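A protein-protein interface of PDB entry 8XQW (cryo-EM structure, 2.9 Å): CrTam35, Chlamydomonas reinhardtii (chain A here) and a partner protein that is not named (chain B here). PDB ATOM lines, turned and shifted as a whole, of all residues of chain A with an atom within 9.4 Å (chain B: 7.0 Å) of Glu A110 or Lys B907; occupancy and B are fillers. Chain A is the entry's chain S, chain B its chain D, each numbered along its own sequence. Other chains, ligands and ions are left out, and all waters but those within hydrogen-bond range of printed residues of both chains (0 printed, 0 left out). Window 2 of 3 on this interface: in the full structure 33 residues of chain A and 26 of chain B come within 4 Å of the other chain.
Printed residues of chain B that touch a printed residue of chain A: Lys B904, Thr B905, Lys B907 and Trp B911. Printed residues of chain A that touch a printed residue of chain B: Arg A100, Val A104, Gly A105, Ala A106, TPO A107, Asp A108, Glu A109, Glu A110 and Val A116. Hydrophobic or aromatic side chains of chain A that line the printed part of chain B: Val A116. Among the printed residues, 11 pairs touch across the chains.
The side-chain amino group of Lys B904 lies within hydrogen-bond range of the backbone carbonyl oxygen of Gly A105, 3.4 Å away. O of TPO A107 is in hydrogen-bond range of N of Thr B905, at 3.4 Å. The side-chain carboxylate (OD1) of Asp A108 lies within salt-bridge range of the side-chain amino group (NZ) of Lys B907 (3.6 Å). The side-chain amino group of Lys B904 lies close to the backbone carbonyl oxygen of Ala A106 (2.3 Å).
NH1 of Arg A100 touches NZ of Lys B904, at 3.9 Å. Val A104 touches Lys B904 (O to NZ, 3.9 Å). Lys B904 touches TPO A107 (CB to O, 3.1 Å). Asp A108 touches Thr B905 (CB to OG1, 3.5 Å). Glu A109 touches Lys B904 (O to NZ, 3.6 Å). Glu A110 touches Lys B907. Trp B911 touches Val A116 (CG to CG1, 3.8 Å).
Of the printed residues of chain B, Arg A100 touches Lys B904 (3.9 Å). Of the printed residues of chain B, Glu A110 touches Lys B907 (3.97 Å). Of the printed residues of chain A, Thr B905 touches TPO A107 and Asp A108. Of chain A, only Asp A108 and Glu A110 come within 4 Å of Lys B907. No residue of chain A comes within 4 Å of Ala B908. His B909 touches none of the printed residues of chain A. The nearest printed residue of chain B that does not touch Val A116 is Lys B910 (7.2 Å).
The guanidinium group (NH1) of Arg A100 is in hydrogen-bond range of the backbone carbonyl oxygen (O) of Gly A105 (3.1 Å). The guanidinium group (NH1) of Arg A100 lies within hydrogen-bond range of the backbone carbonyl oxygen (O) of Ala A106 (2.8 Å). The side-chain carboxylate of Glu A109 sits close to the backbone NH of Val A114 (3.3 Å). The backbone carbonyl oxygen of Trp B911 sits at hydrogen-bond distance from a ring nitrogen (ND1) of His B909, at 3.3 Å.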
ATOM      1  N   ARG A 100     -14.546 -13.100  -5.368  1.00  0.00           N
ATOM      2  CA  ARG A 100     -14.211 -13.585  -6.703  1.00  0.00           C
ATOM      3  C   ARG A 100     -13.800 -15.048  -6.670  1.00  0.00           C
ATOM      4  O   ARG A 100     -14.282 -15.856  -7.469  1.00  0.00           O
ATOM      5  CB  ARG A 100     -13.102 -12.746  -7.324  1.00  0.00           C
ATOM      6  CG  ARG A 100     -12.438 -13.438  -8.501  1.00  0.00           C
ATOM      7  CD  ARG A 100     -11.238 -12.663  -8.997  1.00  0.00           C
ATOM      8  NE  ARG A 100     -10.084 -12.831  -8.128  1.00  0.00           N
ATOM      9  CZ  ARG A 100      -9.260 -13.869  -8.189  1.00  0.00           C
ATOM     10  NH1 ARG A 100      -9.469 -14.824  -9.081  1.00  0.00           N
ATOM     11  NH2 ARG A 100      -8.229 -13.952  -7.362  1.00  0.00           N
ATOM     12  N   THR A 101     -12.895 -15.407  -5.755  1.00  0.00           N
ATOM     13  CA  THR A 101     -12.427 -16.789  -5.692  1.00  0.00           C
ATOM     14  C   THR A 101     -13.577 -17.749  -5.456  1.00  0.00           C
ATOM     15  O   THR A 101     -13.652 -18.795  -6.106  1.00  0.00           O
ATOM     16  CB  THR A 101     -11.383 -16.960  -4.594  1.00  0.00           C
ATOM     17  OG1 THR A 101     -11.770 -16.198  -3.449  1.00  0.00           O
ATOM     18  CG2 THR A 101     -10.028 -16.483  -5.065  1.00  0.00           C
ATOM     19  N   SER A 102     -14.490 -17.401  -4.550  1.00  0.00           N
ATOM     20  CA  SER A 102     -15.639 -18.258  -4.283  1.00  0.00           C
ATOM     21  C   SER A 102     -16.498 -18.444  -5.523  1.00  0.00           C
ATOM     22  O   SER A 102     -16.828 -19.577  -5.891  1.00  0.00           O
ATOM     23  CB  SER A 102     -16.474 -17.672  -3.150  1.00  0.00           C
ATOM     24  OG  SER A 102     -17.854 -17.862  -3.402  1.00  0.00           O
ATOM     25  N   VAL A 103     -16.871 -17.355  -6.185  1.00  0.00           N
ATOM     26  CA  VAL A 103     -17.819 -17.469  -7.289  1.00  0.00           C
ATOM     27  C   VAL A 103     -17.157 -18.000  -8.551  1.00  0.00           C
ATOM     28  O   VAL A 103     -17.488 -19.088  -9.025  1.00  0.00           O
ATOM     29  CB  VAL A 103     -18.499 -16.113  -7.546  1.00  0.00           C
ATOM     30  CG1 VAL A 103     -19.521 -16.254  -8.652  1.00  0.00           C
ATOM     31  CG2 VAL A 103     -19.159 -15.623  -6.282  1.00  0.00           C
ATOM     32  N   VAL A 104     -16.204 -17.258  -9.110  1.00  0.00           N
ATOM     33  CA  VAL A 104     -15.711 -17.501 -10.458  1.00  0.00           C
ATOM     34  C   VAL A 104     -14.368 -18.221 -10.457  1.00  0.00           C
ATOM     35  O   VAL A 104     -13.844 -18.550 -11.519  1.00  0.00           O
ATOM     36  CB  VAL A 104     -15.637 -16.185 -11.259  1.00  0.00           C
ATOM     37  CG1 VAL A 104     -14.429 -15.376 -10.849  1.00  0.00           C
ATOM     38  CG2 VAL A 104     -15.642 -16.451 -12.749  1.00  0.00           C
ATOM     39  N   GLY A 105     -13.807 -18.488  -9.287  1.00  0.00           N
ATOM     40  CA  GLY A 105     -12.599 -19.275  -9.197  1.00  0.00           C
ATOM     41  C   GLY A 105     -11.390 -18.477  -8.749  1.00  0.00           C
ATOM     42  O   GLY A 105     -11.399 -17.250  -8.657  1.00  0.00           O
ATOM     43  N   ALA A 106     -10.318 -19.210  -8.479  1.00  0.00           N
ATOM     44  CA  ALA A 106      -9.100 -18.626  -7.940  1.00  0.00           C
ATOM     45  C   ALA A 106      -8.287 -17.918  -9.011  1.00  0.00           C
ATOM     46  O   ALA A 106      -8.827 -17.434 -10.004  1.00  0.00           O
ATOM     47  CB  ALA A 106      -8.263 -19.692  -7.271  1.00  0.00           C
ATOM     48  N   TPO A 107      -6.976 -17.868  -8.799  1.00  0.00           N
ATOM     49  CA  TPO A 107      -6.082 -17.116  -9.664  1.00  0.00           C
ATOM     50  CB  TPO A 107      -4.924 -16.538  -8.830  1.00  0.00           C
ATOM     51  CG2 TPO A 107      -3.540 -16.768  -9.444  1.00  0.00           C
ATOM     52  OG1 TPO A 107      -5.134 -15.138  -8.640  1.00  0.00           O
ATOM     53  P   TPO A 107      -4.979 -14.867  -7.063  1.00  0.00           P
ATOM     54  O1P TPO A 107      -4.237 -16.113  -6.366  1.00  0.00           O
ATOM     55  O2P TPO A 107      -6.310 -14.691  -6.445  1.00  0.00           O
ATOM     56  O3P TPO A 107      -4.106 -13.538  -6.836  1.00  0.00           O
ATOM     57  C   TPO A 107      -5.564 -17.981 -10.809  1.00  0.00           C
ATOM     58  O   TPO A 107      -5.239 -17.475 -11.882  1.00  0.00           O
ATOM     59  N   ASP A 108      -5.508 -19.288 -10.584  1.00  0.00           N
ATOM     60  CA  ASP A 108      -4.941 -20.204 -11.568  1.00  0.00           C
ATOM     61  C   ASP A 108      -5.759 -21.481 -11.729  1.00  0.00           C
ATOM     62  O   ASP A 108      -5.227 -22.585 -11.626  1.00  0.00           O
ATOM     63  CB  ASP A 108      -3.503 -20.548 -11.186  1.00  0.00           C
ATOM     64  CG  ASP A 108      -3.370 -20.972  -9.738  1.00  0.00           C
ATOM     65  OD1 ASP A 108      -3.608 -22.158  -9.433  1.00  0.00           O
ATOM     66  OD2 ASP A 108      -3.030 -20.111  -8.900  1.00  0.00           O
ATOM     67  N   GLU A 109      -7.053 -21.326 -12.004  1.00  0.00           N
ATOM     68  CA  GLU A 109      -7.920 -22.473 -12.231  1.00  0.00           C
ATOM     69  C   GLU A 109      -9.163 -22.018 -12.978  1.00  0.00           C
ATOM     70  O   GLU A 109      -9.709 -20.951 -12.685  1.00  0.00           O
ATOM     71  CB  GLU A 109      -8.288 -23.147 -10.907  1.00  0.00           C
ATOM     72  CG  GLU A 109      -8.945 -22.236  -9.898  1.00  0.00           C
ATOM     73  CD  GLU A 109      -9.765 -23.000  -8.885  1.00  0.00           C
ATOM     74  OE1 GLU A 109     -10.807 -23.566  -9.272  1.00  0.00           O
ATOM     75  OE2 GLU A 109      -9.368 -23.041  -7.703  1.00  0.00           O
ATOM     76  N   GLU A 110      -9.595 -22.819 -13.945  1.00  0.00           N
ATOM     77  CA  GLU A 110     -10.731 -22.490 -14.790  1.00  0.00           C
ATOM     78  C   GLU A 110     -12.027 -22.883 -14.086  1.00  0.00           C
ATOM     79  O   GLU A 110     -12.050 -23.150 -12.882  1.00  0.00           O
ATOM     80  CB  GLU A 110     -10.598 -23.178 -16.145  1.00  0.00           C
ATOM     81  CG  GLU A 110      -9.426 -22.697 -16.976  1.00  0.00           C
ATOM     82  CD  GLU A 110      -8.964 -23.733 -17.983  1.00  0.00           C
ATOM     83  OE1 GLU A 110      -7.775 -23.707 -18.361  1.00  0.00           O
ATOM     84  OE2 GLU A 110      -9.788 -24.578 -18.386  1.00  0.00           O
ATOM     85  N   LEU A 111     -13.132 -22.908 -14.831  1.00  0.00           N
ATOM     86  CA  LEU A 111     -14.409 -23.296 -14.246  1.00  0.00           C
ATOM     87  C   LEU A 111     -14.466 -24.784 -13.928  1.00  0.00           C
ATOM     88  O   LEU A 111     -15.079 -25.176 -12.929  1.00  0.00           O
ATOM     89  CB  LEU A 111     -15.553 -22.912 -15.184  1.00  0.00           C
ATOM     90  CG  LEU A 111     -15.979 -21.445 -15.107  1.00  0.00           C
ATOM     91  CD1 LEU A 111     -17.142 -21.154 -16.039  1.00  0.00           C
ATOM     92  CD2 LEU A 111     -16.338 -21.075 -13.685  1.00  0.00           C
ATOM     93  N   GLU A 112     -13.839 -25.622 -14.757  1.00  0.00           N
ATOM     94  CA  GLU A 112     -13.823 -27.053 -14.481  1.00  0.00           C
ATOM     95  C   GLU A 112     -13.182 -27.352 -13.137  1.00  0.00           C
ATOM     96  O   GLU A 112     -13.621 -28.263 -12.427  1.00  0.00           O
ATOM     97  CB  GLU A 112     -13.075 -27.795 -15.585  1.00  0.00           C
ATOM     98  CG  GLU A 112     -13.767 -27.786 -16.929  1.00  0.00           C
ATOM     99  CD  GLU A 112     -13.459 -26.537 -17.725  1.00  0.00           C
ATOM    100  OE1 GLU A 112     -13.436 -25.442 -17.127  1.00  0.00           O
ATOM    101  OE2 GLU A 112     -13.220 -26.653 -18.945  1.00  0.00           O
ATOM    102  N   ASP A 113     -12.146 -26.600 -12.770  1.00  0.00           N
ATOM    103  CA  ASP A 113     -11.482 -26.859 -11.501  1.00  0.00           C
ATOM    104  C   ASP A 113     -12.371 -26.461 -10.332  1.00  0.00           C
ATOM    105  O   ASP A 113     -12.359 -27.115  -9.286  1.00  0.00           O
ATOM    106  CB  ASP A 113     -10.146 -26.132 -11.459  1.00  0.00           C
ATOM    107  CG  ASP A 113      -9.334 -26.360 -12.714  1.00  0.00           C
ATOM    108  OD1 ASP A 113      -9.925 -26.805 -13.718  1.00  0.00           O
ATOM    109  OD2 ASP A 113      -8.113 -26.098 -12.697  1.00  0.00           O
ATOM    110  N   VAL A 114     -13.194 -25.429 -10.509  1.00  0.00           N
ATOM    111  CA  VAL A 114     -14.180 -25.102  -9.486  1.00  0.00           C
ATOM    112  C   VAL A 114     -15.227 -26.203  -9.386  1.00  0.00           C
ATOM    113  O   VAL A 114     -15.657 -26.571  -8.284  1.00  0.00           O
ATOM    114  CB  VAL A 114     -14.822 -23.734  -9.776  1.00  0.00           C
ATOM    115  CG1 VAL A 114     -16.120 -23.586  -9.018  1.00  0.00           C
ATOM    116  CG2 VAL A 114     -13.872 -22.639  -9.380  1.00  0.00           C
ATOM    117  N   ALA A 115     -15.653 -26.748 -10.526  1.00  0.00           N
ATOM    118  CA  ALA A 115     -16.645 -27.819 -10.495  1.00  0.00           C
ATOM    119  C   ALA A 115     -16.111 -29.044  -9.771  1.00  0.00           C
ATOM    120  O   ALA A 115     -16.816 -29.650  -8.961  1.00  0.00           O
ATOM    121  CB  ALA A 115     -17.078 -28.186 -11.911  1.00  0.00           C
ATOM    122  N   VAL A 116     -14.863 -29.423 -10.043  1.00  0.00           N
ATOM    123  CA  VAL A 116     -14.293 -30.580  -9.358  1.00  0.00           C
ATOM    124  C   VAL A 116     -13.941 -30.237  -7.916  1.00  0.00           C
ATOM    125  O   VAL A 116     -13.738 -31.129  -7.089  1.00  0.00           O
ATOM    126  CB  VAL A 116     -13.072 -31.120 -10.121  1.00  0.00           C
ATOM    127  CG1 VAL A 116     -13.399 -31.290 -11.583  1.00  0.00           C
ATOM    128  CG2 VAL A 116     -11.882 -30.208  -9.934  1.00  0.00           C
ATOM    129  N   ARG A 117     -13.848 -28.949  -7.590  1.00  0.00           N
ATOM    130  CA  ARG A 117     -13.626 -28.581  -6.199  1.00  0.00           C
ATOM    131  C   ARG A 117     -14.902 -28.711  -5.383  1.00  0.00           C
ATOM    132  O   ARG A 117     -14.878 -29.247  -4.272  1.00  0.00           O
ATOM    133  CB  ARG A 117     -13.078 -27.159  -6.108  1.00  0.00           C
ATOM    134  CG  ARG A 117     -12.732 -26.719  -4.701  1.00  0.00           C
ATOM    135  CD  ARG A 117     -13.541 -25.507  -4.286  1.00  0.00           C
ATOM    136  NE  ARG A 117     -13.404 -24.408  -5.236  1.00  0.00           N
ATOM    137  CZ  ARG A 117     -14.110 -23.282  -5.186  1.00  0.00           C
ATOM    138  NH1 ARG A 117     -15.002 -23.096  -4.224  1.00  0.00           N
ATOM    139  NH2 ARG A 117     -13.919 -22.336  -6.096  1.00  0.00           N
ATOM    140  N   LYS B 904      -6.280 -15.096 -15.640  1.00  0.00           N
ATOM    141  CA  LYS B 904      -5.684 -16.191 -14.895  1.00  0.00           C
ATOM    142  C   LYS B 904      -4.491 -16.785 -15.636  1.00  0.00           C
ATOM    143  O   LYS B 904      -4.419 -16.767 -16.867  1.00  0.00           O
ATOM    144  CB  LYS B 904      -6.730 -17.282 -14.640  1.00  0.00           C
ATOM    145  CG  LYS B 904      -7.942 -16.791 -13.861  1.00  0.00           C
ATOM    146  CD  LYS B 904      -9.169 -17.651 -14.123  1.00  0.00           C
ATOM    147  CE  LYS B 904     -10.350 -17.194 -13.282  1.00  0.00           C
ATOM    148  NZ  LYS B 904     -10.152 -17.475 -11.837  1.00  0.00           N
ATOM    149  N   THR B 905      -3.559 -17.331 -14.857  1.00  0.00           N
ATOM    150  CA  THR B 905      -2.387 -18.029 -15.381  1.00  0.00           C
ATOM    151  C   THR B 905      -2.822 -19.437 -15.765  1.00  0.00           C
ATOM    152  O   THR B 905      -3.028 -20.303 -14.915  1.00  0.00           O
ATOM    153  CB  THR B 905      -1.267 -18.059 -14.351  1.00  0.00           C
ATOM    154  OG1 THR B 905      -1.365 -19.261 -13.578  1.00  0.00           O
ATOM    155  CG2 THR B 905      -1.378 -16.865 -13.416  1.00  0.00           C
ATOM    156  N   LEU B 906      -2.961 -19.668 -17.064  1.00  0.00           N
ATOM    157  CA  LEU B 906      -3.561 -20.887 -17.576  1.00  0.00           C
ATOM    158  C   LEU B 906      -2.522 -21.977 -17.810  1.00  0.00           C
ATOM    159  O   LEU B 906      -1.368 -21.704 -18.149  1.00  0.00           O
ATOM    160  CB  LEU B 906      -4.316 -20.586 -18.872  1.00  0.00           C
ATOM    161  CG  LEU B 906      -3.670 -19.555 -19.806  1.00  0.00           C
ATOM    162  CD1 LEU B 906      -2.722 -20.207 -20.804  1.00  0.00           C
ATOM    163  CD2 LEU B 906      -4.735 -18.737 -20.523  1.00  0.00           C
ATOM    164  N   LYS B 907      -2.950 -23.223 -17.617  1.00  0.00           N
ATOM    165  CA  LYS B 907      -2.131 -24.399 -17.890  1.00  0.00           C
ATOM    166  C   LYS B 907      -3.064 -25.582 -18.128  1.00  0.00           C
ATOM    167  O   LYS B 907      -4.272 -25.503 -17.885  1.00  0.00           O
ATOM    168  CB  LYS B 907      -1.138 -24.668 -16.754  1.00  0.00           C
ATOM    169  CG  LYS B 907      -1.724 -25.397 -15.559  1.00  0.00           C
ATOM    170  CD  LYS B 907      -2.259 -24.429 -14.521  1.00  0.00           C
ATOM    171  CE  LYS B 907      -2.987 -25.170 -13.415  1.00  0.00           C
ATOM    172  NZ  LYS B 907      -3.580 -24.241 -12.416  1.00  0.00           N
ATOM    173  N   ALA B 908      -2.491 -26.688 -18.601  1.00  0.00           N
ATOM    174  CA  ALA B 908      -3.291 -27.841 -18.998  1.00  0.00           C
ATOM    175  C   ALA B 908      -3.981 -28.476 -17.796  1.00  0.00           C
ATOM    176  O   ALA B 908      -3.372 -28.687 -16.744  1.00  0.00           O
ATOM    177  CB  ALA B 908      -2.416 -28.875 -19.706  1.00  0.00           C
ATOM    178  N   HIS B 909      -5.260 -28.794 -17.968  1.00  0.00           N
ATOM    179  CA  HIS B 909      -6.089 -29.372 -16.923  1.00  0.00           C
ATOM    180  C   HIS B 909      -6.022 -30.894 -16.972  1.00  0.00           C
ATOM    181  O   HIS B 909      -5.234 -31.489 -17.708  1.00  0.00           O
ATOM    182  CB  HIS B 909      -7.533 -28.885 -17.061  1.00  0.00           C
ATOM    183  CG  HIS B 909      -8.146 -29.175 -18.396  1.00  0.00           C
ATOM    184  ND1 HIS B 909      -9.319 -28.587 -18.816  1.00  0.00           N
ATOM    185  CD2 HIS B 909      -7.752 -29.990 -19.402  1.00  0.00           C
ATOM    186  CE1 HIS B 909      -9.620 -29.026 -20.025  1.00  0.00           C
ATOM    187  NE2 HIS B 909      -8.687 -29.879 -20.403  1.00  0.00           N
ATOM    188  N   LYS B 910      -6.872 -31.532 -16.172  1.00  0.00           N
ATOM    189  CA  LYS B 910      -6.946 -32.986 -16.168  1.00  0.00           C
ATOM    190  C   LYS B 910      -8.389 -33.445 -16.317  1.00  0.00           C
ATOM    191  O   LYS B 910      -8.656 -34.508 -16.888  1.00  0.00           O
ATOM    192  CB  LYS B 910      -6.323 -33.546 -14.887  1.00  0.00           C
ATOM    193  CG  LYS B 910      -5.980 -35.019 -14.960  1.00  0.00           C
ATOM    194  CD  LYS B 910      -4.722 -35.273 -15.781  1.00  0.00           C
ATOM    195  CE  LYS B 910      -3.675 -34.185 -15.591  1.00  0.00           C
ATOM    196  NZ  LYS B 910      -2.571 -34.318 -16.579  1.00  0.00           N
ATOM    197  N   TRP B 911      -9.324 -32.646 -15.814  1.00  0.00           N
ATOM    198  CA  TRP B 911     -10.746 -32.915 -15.936  1.00  0.00           C
ATOM    199  C   TRP B 911     -11.328 -32.066 -17.054  1.00  0.00           C
ATOM    200  O   TRP B 911     -11.017 -30.878 -17.172  1.00  0.00           O
ATOM    201  CB  TRP B 911     -11.482 -32.620 -14.632  1.00  0.00           C
ATOM    202  CG  TRP B 911     -11.473 -33.759 -13.685  1.00  0.00           C
ATOM    203  CD1 TRP B 911     -10.534 -34.027 -12.740  1.00  0.00           C
ATOM    204  CD2 TRP B 911     -12.447 -34.800 -13.593  1.00  0.00           C
ATOM    205  NE1 TRP B 911     -10.863 -35.170 -12.059  1.00  0.00           N
ATOM    206  CE2 TRP B 911     -12.037 -35.663 -12.562  1.00  0.00           C
ATOM    207  CE3 TRP B 911     -13.630 -35.084 -14.279  1.00  0.00           C
ATOM    208  CZ2 TRP B 911     -12.763 -36.792 -12.203  1.00  0.00           C
ATOM    209  CZ3 TRP B 911     -14.350 -36.205 -13.920  1.00  0.00           C
ATOM    210  CH2 TRP B 911     -13.915 -37.046 -12.891  1.00  0.00           C
